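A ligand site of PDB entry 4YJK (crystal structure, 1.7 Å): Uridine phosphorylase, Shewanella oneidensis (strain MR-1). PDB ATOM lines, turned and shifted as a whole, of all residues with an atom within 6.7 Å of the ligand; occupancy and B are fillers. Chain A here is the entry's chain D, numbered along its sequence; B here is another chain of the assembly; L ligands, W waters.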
ATOM      1  N   ARG A  89     -45.065  18.023  -8.620  1.00  0.00           N
ATOM      2  CA  ARG A  89     -43.735  17.866  -8.090  1.00  0.00           C
ATOM      3  C   ARG A  89     -42.880  18.932  -8.740  1.00  0.00           C
ATOM      4  O   ARG A  89     -43.018  19.138  -9.944  1.00  0.00           O
ATOM      5  CB  ARG A  89     -43.155  16.469  -8.439  1.00  0.00           C
ATOM      6  CG  ARG A  89     -41.641  16.412  -8.280  1.00  0.00           C
ATOM      7  CD  ARG A  89     -41.009  15.048  -8.430  1.00  0.00           C
ATOM      8  NE  ARG A  89     -39.613  15.193  -8.907  1.00  0.00           N
ATOM      9  CZ  ARG A  89     -38.583  15.580  -8.157  1.00  0.00           C
ATOM     10  NH1 ARG A  89     -38.739  15.898  -6.872  1.00  0.00           N
ATOM     11  NH2 ARG A  89     -37.363  15.676  -8.697  1.00  0.00           N
ATOM     12  N   THR A  92     -35.108  18.988  -8.794  1.00  0.00           N
ATOM     13  CA  THR A  92     -33.831  19.246  -9.485  1.00  0.00           C
ATOM     14  C   THR A  92     -33.476  17.936 -10.160  1.00  0.00           C
ATOM     15  O   THR A  92     -33.997  16.905  -9.770  1.00  0.00           O
ATOM     16  CB  THR A  92     -32.706  19.606  -8.547  1.00  0.00           C
ATOM     17  OG1 THR A  92     -32.421  18.493  -7.683  1.00  0.00           O
ATOM     18  CG2 THR A  92     -33.066  20.870  -7.764  1.00  0.00           C
ATOM     19  N   THR A  93     -32.573  17.961 -11.142  1.00  0.00           N
ATOM     20  CA  THR A  93     -32.428  16.804 -12.008  1.00  0.00           C
ATOM     21  C   THR A  93     -31.052  16.935 -12.705  1.00  0.00           C
ATOM     22  O   THR A  93     -30.528  18.027 -12.790  1.00  0.00           O
ATOM     23  CB  THR A  93     -33.558  16.658 -13.051  1.00  0.00           C
ATOM     24  OG1 THR A  93     -33.478  15.358 -13.652  1.00  0.00           O
ATOM     25  CG2 THR A  93     -33.482  17.713 -14.146  1.00  0.00           C
ATOM     26  N   GLY A  94     -30.507  15.775 -13.066  1.00  0.00           N
ATOM     27  CA  GLY A  94     -29.301  15.664 -13.872  1.00  0.00           C
ATOM     28  C   GLY A  94     -29.709  15.315 -15.304  1.00  0.00           C
ATOM     29  O   GLY A  94     -30.297  14.218 -15.570  1.00  0.00           O
ATOM     30  N   ALA A  95     -29.324  16.140 -16.286  1.00  0.00           N
ATOM     31  CA  ALA A  95     -29.570  15.808 -17.703  1.00  0.00           C
ATOM     32  C   ALA A  95     -28.611  14.726 -18.203  1.00  0.00           C
ATOM     33  O   ALA A  95     -27.435  14.673 -17.822  1.00  0.00           O
ATOM     34  CB  ALA A  95     -29.427  17.047 -18.556  1.00  0.00           C
ATOM     35  N   ALA A 155     -35.556   8.947 -16.487  1.00  0.00           N
ATOM     36  CA  ALA A 155     -35.138   7.804 -15.741  1.00  0.00           C
ATOM     37  C   ALA A 155     -35.216   8.087 -14.194  1.00  0.00           C
ATOM     38  O   ALA A 155     -34.589   8.995 -13.664  1.00  0.00           O
ATOM     39  CB  ALA A 155     -33.680   7.494 -16.177  1.00  0.00           C
ATOM     40  N   SER A 157     -34.738   6.744 -10.636  1.00  0.00           N
ATOM     41  CA  SER A 157     -33.921   5.712  -9.997  1.00  0.00           C
ATOM     42  C   SER A 157     -34.014   5.736  -8.457  1.00  0.00           C
ATOM     43  O   SER A 157     -33.993   6.797  -7.775  1.00  0.00           O
ATOM     44  CB  SER A 157     -32.432   5.874 -10.463  1.00  0.00           C
ATOM     45  OG  SER A 157     -31.544   5.316  -9.531  1.00  0.00           O
ATOM     46  N   THR A 159     -31.608   4.977  -6.625  1.00  0.00           N
ATOM     47  CA  THR A 159     -30.359   5.439  -6.066  1.00  0.00           C
ATOM     48  C   THR A 159     -29.841   6.619  -6.879  1.00  0.00           C
ATOM     49  O   THR A 159     -30.206   6.801  -8.024  1.00  0.00           O
ATOM     50  CB  THR A 159     -29.270   4.355  -6.007  1.00  0.00           C
ATOM     51  OG1 THR A 159     -28.909   3.926  -7.328  1.00  0.00           O
ATOM     52  CG2 THR A 159     -29.708   3.166  -5.149  1.00  0.00           C
ATOM     53  N   PHE A 160     -28.946   7.346  -6.270  1.00  0.00           N
ATOM     54  CA  PHE A 160     -28.293   8.516  -6.855  1.00  0.00           C
ATOM     55  C   PHE A 160     -26.976   8.082  -7.439  1.00  0.00           C
ATOM     56  O   PHE A 160     -26.534   8.706  -8.364  1.00  0.00           O
ATOM     57  CB  PHE A 160     -27.969   9.546  -5.745  1.00  0.00           C
ATOM     58  CG  PHE A 160     -27.361  10.857  -6.252  1.00  0.00           C
ATOM     59  CD1 PHE A 160     -28.155  11.908  -6.736  1.00  0.00           C
ATOM     60  CD2 PHE A 160     -25.994  11.060  -6.186  1.00  0.00           C
ATOM     61  CE1 PHE A 160     -27.594  13.096  -7.195  1.00  0.00           C
ATOM     62  CE2 PHE A 160     -25.423  12.255  -6.666  1.00  0.00           C
ATOM     63  CZ  PHE A 160     -26.222  13.257  -7.166  1.00  0.00           C
ATOM     64  N   GLN A 164     -27.774   5.693 -11.280  1.00  0.00           N
ATOM     65  CA  GLN A 164     -27.526   6.770 -12.217  1.00  0.00           C
ATOM     66  C   GLN A 164     -26.103   6.625 -12.729  1.00  0.00           C
ATOM     67  O   GLN A 164     -25.548   7.592 -13.323  1.00  0.00           O
ATOM     68  CB  GLN A 164     -27.746   8.122 -11.522  1.00  0.00           C
ATOM     69  CG  GLN A 164     -29.154   8.230 -10.928  1.00  0.00           C
ATOM     70  CD  GLN A 164     -29.495   9.606 -10.400  1.00  0.00           C
ATOM     71  OE1 GLN A 164     -29.023  10.649 -10.909  1.00  0.00           O
ATOM     72  NE2 GLN A 164     -30.445   9.651  -9.427  1.00  0.00           N
ATOM     73  N   ARG A 166     -23.137   6.460 -11.663  1.00  0.00           N
ATOM     74  CA  ARG A 166     -22.013   7.217 -11.104  1.00  0.00           C
ATOM     75  C   ARG A 166     -20.910   6.270 -10.607  1.00  0.00           C
ATOM     76  O   ARG A 166     -21.180   5.318  -9.934  1.00  0.00           O
ATOM     77  CB  ARG A 166     -22.456   8.140  -9.992  1.00  0.00           C
ATOM     78  CG  ARG A 166     -23.291   9.323 -10.466  1.00  0.00           C
ATOM     79  CD  ARG A 166     -23.570  10.268  -9.331  1.00  0.00           C
ATOM     80  NE  ARG A 166     -24.009  11.539  -9.834  1.00  0.00           N
ATOM     81  CZ  ARG A 166     -25.258  11.914 -10.025  1.00  0.00           C
ATOM     82  NH1 ARG A 166     -26.274  11.180  -9.625  1.00  0.00           N
ATOM     83  NH2 ARG A 166     -25.477  13.074 -10.556  1.00  0.00           N
ATOM     84  N   TYR A 193     -32.163  12.059 -15.236  1.00  0.00           N
ATOM     85  CA  TYR A 193     -32.337  11.273 -14.007  1.00  0.00           C
ATOM     86  C   TYR A 193     -32.940  12.064 -12.871  1.00  0.00           C
ATOM     87  O   TYR A 193     -32.545  13.196 -12.633  1.00  0.00           O
ATOM     88  CB  TYR A 193     -30.967  10.807 -13.492  1.00  0.00           C
ATOM     89  CG  TYR A 193     -30.349   9.601 -14.180  1.00  0.00           C
ATOM     90  CD1 TYR A 193     -30.951   8.352 -14.177  1.00  0.00           C
ATOM     91  CD2 TYR A 193     -29.070   9.689 -14.794  1.00  0.00           C
ATOM     92  CE1 TYR A 193     -30.379   7.250 -14.785  1.00  0.00           C
ATOM     93  CE2 TYR A 193     -28.466   8.555 -15.352  1.00  0.00           C
ATOM     94  CZ  TYR A 193     -29.104   7.365 -15.391  1.00  0.00           C
ATOM     95  OH  TYR A 193     -28.506   6.253 -15.950  1.00  0.00           O
ATOM     96  N   GLU A 194     -33.943  11.464 -12.179  1.00  0.00           N
ATOM     97  CA  GLU A 194     -34.440  11.972 -10.883  1.00  0.00           C
ATOM     98  C   GLU A 194     -34.789  10.756  -9.997  1.00  0.00           C
ATOM     99  O   GLU A 194     -34.450   9.636 -10.386  1.00  0.00           O
ATOM    100  CB  GLU A 194     -35.806  12.727 -11.061  1.00  0.00           C
ATOM    101  CG  GLU A 194     -35.993  13.624 -12.293  1.00  0.00           C
ATOM    102  CD  GLU A 194     -37.147  14.613 -12.231  1.00  0.00           C
ATOM    103  OE1 GLU A 194     -38.017  14.577 -11.327  1.00  0.00           O
ATOM    104  OE2 GLU A 194     -37.179  15.460 -13.141  1.00  0.00           O
ATOM    105  N   MET A 195     -35.418  10.947  -8.845  1.00  0.00           N
ATOM    106  CA  MET A 195     -35.547   9.791  -7.965  1.00  0.00           C
ATOM    107  C   MET A 195     -36.945   9.538  -7.478  1.00  0.00           C
ATOM    108  O   MET A 195     -37.160   8.607  -6.724  1.00  0.00           O
ATOM    109  CB  MET A 195     -34.588   9.813  -6.799  1.00  0.00           C
ATOM    110  CG  MET A 195     -33.103   9.931  -7.297  1.00  0.00           C
ATOM    111  SD  MET A 195     -31.893   9.908  -5.989  1.00  0.00           S
ATOM    112  CE  MET A 195     -32.272   8.382  -5.145  1.00  0.00           C
ATOM    113  N   GLU A 196     -37.858  10.372  -7.855  1.00  0.00           N
ATOM    114  CA  GLU A 196     -39.238  10.195  -7.312  1.00  0.00           C
ATOM    115  C   GLU A 196     -40.404   9.952  -8.317  1.00  0.00           C
ATOM    116  O   GLU A 196     -41.434   9.414  -7.909  1.00  0.00           O
ATOM    117  CB  GLU A 196     -39.602  11.435  -6.525  1.00  0.00           C
ATOM    118  CG  GLU A 196     -38.740  11.691  -5.314  1.00  0.00           C
ATOM    119  CD  GLU A 196     -37.357  12.276  -5.648  1.00  0.00           C
ATOM    120  OE1 GLU A 196     -37.248  12.900  -6.722  1.00  0.00           O
ATOM    121  OE2 GLU A 196     -36.444  12.122  -4.822  1.00  0.00           O
ATOM    122  N   GLY A 216     -35.697  21.476 -12.520  1.00  0.00           N
ATOM    123  CA  GLY A 216     -34.550  22.276 -13.016  1.00  0.00           C
ATOM    124  C   GLY A 216     -33.312  21.476 -13.131  1.00  0.00           C
ATOM    125  O   GLY A 216     -32.967  20.723 -12.254  1.00  0.00           O
ATOM    126  N   ILE A 218     -29.580  20.802 -12.893  1.00  0.00           N
ATOM    127  CA  ILE A 218     -28.440  21.229 -12.079  1.00  0.00           C
ATOM    128  C   ILE A 218     -27.071  20.686 -12.518  1.00  0.00           C
ATOM    129  O   ILE A 218     -26.088  21.194 -12.036  1.00  0.00           O
ATOM    130  CB  ILE A 218     -28.645  21.036 -10.584  1.00  0.00           C
ATOM    131  CG1 ILE A 218     -28.769  19.559 -10.110  1.00  0.00           C
ATOM    132  CG2 ILE A 218     -29.916  21.800 -10.149  1.00  0.00           C
ATOM    133  CD1 ILE A 218     -28.536  19.324  -8.605  1.00  0.00           C
ATOM    134  N   VAL A 219     -27.057  19.669 -13.390  1.00  0.00           N
ATOM    135  CA  VAL A 219     -25.840  19.029 -13.867  1.00  0.00           C
ATOM    136  C   VAL A 219     -26.180  18.361 -15.192  1.00  0.00           C
ATOM    137  O   VAL A 219     -27.288  17.940 -15.385  1.00  0.00           O
ATOM    138  CB  VAL A 219     -25.252  18.024 -12.880  1.00  0.00           C
ATOM    139  CG1 VAL A 219     -26.140  16.791 -12.753  1.00  0.00           C
ATOM    140  CG2 VAL A 219     -23.850  17.606 -13.326  1.00  0.00           C
ATOM    141  N   ARG A 221     -24.816  15.172 -17.137  1.00  0.00           N
ATOM    142  CA  ARG A 221     -24.032  13.995 -16.887  1.00  0.00           C
ATOM    143  C   ARG A 221     -23.085  13.631 -18.017  1.00  0.00           C
ATOM    144  O   ARG A 221     -22.182  12.912 -17.789  1.00  0.00           O
ATOM    145  CB  ARG A 221     -24.947  12.809 -16.597  1.00  0.00           C
ATOM    146  CG  ARG A 221     -25.666  13.044 -15.250  1.00  0.00           C
ATOM    147  CD  ARG A 221     -24.795  12.955 -13.996  1.00  0.00           C
ATOM    148  NE  ARG A 221     -23.903  11.792 -14.110  1.00  0.00           N
ATOM    149  CZ  ARG A 221     -24.246  10.534 -13.856  1.00  0.00           C
ATOM    150  NH1 ARG A 221     -25.442  10.248 -13.369  1.00  0.00           N
ATOM    151  NH2 ARG A 221     -23.384   9.584 -14.031  1.00  0.00           N
ATOM    152  N   GLU A 225     -20.274  14.266 -13.269  1.00  0.00           N
ATOM    153  CA  GLU A 225     -21.127  13.432 -12.366  1.00  0.00           C
ATOM    154  C   GLU A 225     -21.846  14.205 -11.294  1.00  0.00           C
ATOM    155  O   GLU A 225     -22.943  13.810 -10.900  1.00  0.00           O
ATOM    156  CB  GLU A 225     -20.315  12.354 -11.644  1.00  0.00           C
ATOM    157  CG  GLU A 225     -20.160  11.098 -12.471  1.00  0.00           C
ATOM    158  CD  GLU A 225     -19.691   9.893 -11.749  1.00  0.00           C
ATOM    159  OE1 GLU A 225     -19.549   9.819 -10.487  1.00  0.00           O
ATOM    160  OE2 GLU A 225     -19.413   8.932 -12.488  1.00  0.00           O
ATOM    161  N   PRO A 227     -22.386  18.427  -9.794  1.00  0.00           N
ATOM    162  CA  PRO A 227     -22.014  19.783 -10.197  1.00  0.00           C
ATOM    163  C   PRO A 227     -21.166  20.477  -9.154  1.00  0.00           C
ATOM    164  O   PRO A 227     -21.197  20.099  -7.995  1.00  0.00           O
ATOM    165  CB  PRO A 227     -23.359  20.498 -10.329  1.00  0.00           C
ATOM    166  CG  PRO A 227     -24.268  19.747  -9.403  1.00  0.00           C
ATOM    167  CD  PRO A 227     -23.762  18.363  -9.229  1.00  0.00           C
ATOM    168  N   PHE B   5     -21.873  15.458  -1.807  1.00  0.00           N
ATOM    169  CA  PHE B   5     -22.900  16.313  -2.389  1.00  0.00           C
ATOM    170  C   PHE B   5     -24.148  16.608  -1.570  1.00  0.00           C
ATOM    171  O   PHE B   5     -24.677  17.681  -1.701  1.00  0.00           O
ATOM    172  CB  PHE B   5     -23.319  15.713  -3.722  1.00  0.00           C
ATOM    173  CG  PHE B   5     -24.167  16.622  -4.543  1.00  0.00           C
ATOM    174  CD1 PHE B   5     -23.700  17.878  -4.920  1.00  0.00           C
ATOM    175  CD2 PHE B   5     -25.412  16.239  -4.907  1.00  0.00           C
ATOM    176  CE1 PHE B   5     -24.493  18.701  -5.699  1.00  0.00           C
ATOM    177  CE2 PHE B   5     -26.206  17.042  -5.697  1.00  0.00           C
ATOM    178  CZ  PHE B   5     -25.757  18.294  -6.067  1.00  0.00           C
ATOM    179  N   HIS B   6     -24.633  15.678  -0.761  1.00  0.00           N
ATOM    180  CA  HIS B   6     -25.880  15.870   0.002  1.00  0.00           C
ATOM    181  C   HIS B   6     -25.691  16.147   1.511  1.00  0.00           C
ATOM    182  O   HIS B   6     -26.419  16.983   2.071  1.00  0.00           O
ATOM    183  CB  HIS B   6     -26.759  14.608  -0.152  1.00  0.00           C
ATOM    184  CG  HIS B   6     -27.226  14.369  -1.529  1.00  0.00           C
ATOM    185  ND1 HIS B   6     -26.511  13.571  -2.408  1.00  0.00           N
ATOM    186  CD2 HIS B   6     -28.337  14.773  -2.203  1.00  0.00           C
ATOM    187  CE1 HIS B   6     -27.171  13.492  -3.550  1.00  0.00           C
ATOM    188  NE2 HIS B   6     -28.288  14.199  -3.446  1.00  0.00           N
ATOM    189  N   ARG B  46     -31.526  18.838   3.881  1.00  0.00           N
ATOM    190  CA  ARG B  46     -32.615  17.955   3.496  1.00  0.00           C
ATOM    191  C   ARG B  46     -32.915  17.129   4.751  1.00  0.00           C
ATOM    192  O   ARG B  46     -32.918  17.685   5.819  1.00  0.00           O
ATOM    193  CB  ARG B  46     -32.219  17.046   2.315  1.00  0.00           C
ATOM    194  CG  ARG B  46     -31.928  17.798   1.025  1.00  0.00           C
ATOM    195  CD  ARG B  46     -31.711  16.837  -0.106  1.00  0.00           C
ATOM    196  NE  ARG B  46     -31.554  17.428  -1.408  1.00  0.00           N
ATOM    197  CZ  ARG B  46     -32.510  17.466  -2.367  1.00  0.00           C
ATOM    198  NH1 ARG B  46     -33.763  17.017  -2.114  1.00  0.00           N
ATOM    199  NH2 ARG B  46     -32.206  17.988  -3.542  1.00  0.00           N
HETATM  200  N1  LIG L   1     -31.367  14.506  -8.762  1.00  0.00           N
HETATM  201  C1  LIG L   1     -31.018  13.254  -9.226  1.00  0.00           C
HETATM  202  O1  LIG L   1     -31.639  12.241  -8.942  1.00  0.00           O
HETATM  203  N2  LIG L   1     -29.877  13.222 -10.004  1.00  0.00           N
HETATM  204  C2  LIG L   1     -29.095  14.282 -10.380  1.00  0.00           C
HETATM  205  O2  LIG L   1     -28.094  14.094 -11.085  1.00  0.00           O
HETATM  206  C3  LIG L   1     -29.522  15.552  -9.854  1.00  0.00           C
HETATM  207  C4  LIG L   1     -30.614  15.624  -9.094  1.00  0.00           C
HETATM  208  O   HOH W   1     -27.724  12.029 -12.748  1.00  0.00           O
HETATM  209  O   HOH W   2     -30.319  17.362  -6.241  1.00  0.00           O
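The side-chain amide oxygen (OE1) of Gln 164 lies within hydrogen-bond range of the guanidinium group (NH1) of Arg 166 (3.1 Å). NH1 of Arg 221 sits at hydrogen-bond distance from O of Gln 164, 2.7 Å away. The side-chain amide nitrogen (NE2) of Gln 164 lies within hydrogen-bond range of the backbone carbonyl oxygen (O) of Thr 159 (3.2 Å). The backbone carbonyl oxygen (O) of Gly 94 sits at hydrogen-bond distance from the backbone NH (N) of Tyr 193, 2.9 Å away. The backbone carbonyl oxygen of Glu 194 sits at hydrogen-bond distance from the backbone NH of Ser 157 (2.9 Å). OE1 of Glu 194 is in salt-bridge range of NH2 of Arg 89. N of Glu 194 lies within hydrogen-bond range of O of Ala 155, at 3.0 Å. The backbone carbonyl oxygen of Thr 93 lies within hydrogen-bond range of the backbone NH of Ile 218, at 2.9 Å.
Water W1 lies within hydrogen-bond range of OE1 of Gln 164 (2.6 Å), O2 of the ligand (2.7 Å), NH1 of Arg 221 (3.0 Å) and NH2 of Arg 166 (3.3 Å). Water W2 lies within hydrogen-bond range of OG1 of Thr 92 (2.8 Å) and NH2 of Arg 46 of chain B (3.4 Å).
An oxygen (O1) of the ligand lies close to the side-chain sulfur of Met 195, at 3.8 Å. Residues that only touch the ligand: Thr 92 (3.7 Å), Thr 93 (3.5 Å), Gly 94 (3.4 Å), Phe 160 (3.6 Å), Tyr 193 (3.7 Å), Glu 194 (3.4 Å) and Val 219 (3.7 Å). Hydrophobic or aromatic side chains within 4 Å of the ligand: Phe 160, Met 195 and Val 219. Of the 24 residues printed, 10 come within 4 Å of the ligand. The nearest printed residue that does not touch the ligand is Ile 218 (4.1 Å).
The side-chain amide oxygen (OE1) of Gln 164 is in hydrogen-bond range of a nitrogen (N2) of the ligand (2.9 Å). The guanidinium group of Arg 166 lies within hydrogen-bond range of an oxygen (O2) of the ligand, 2.9 Å away.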
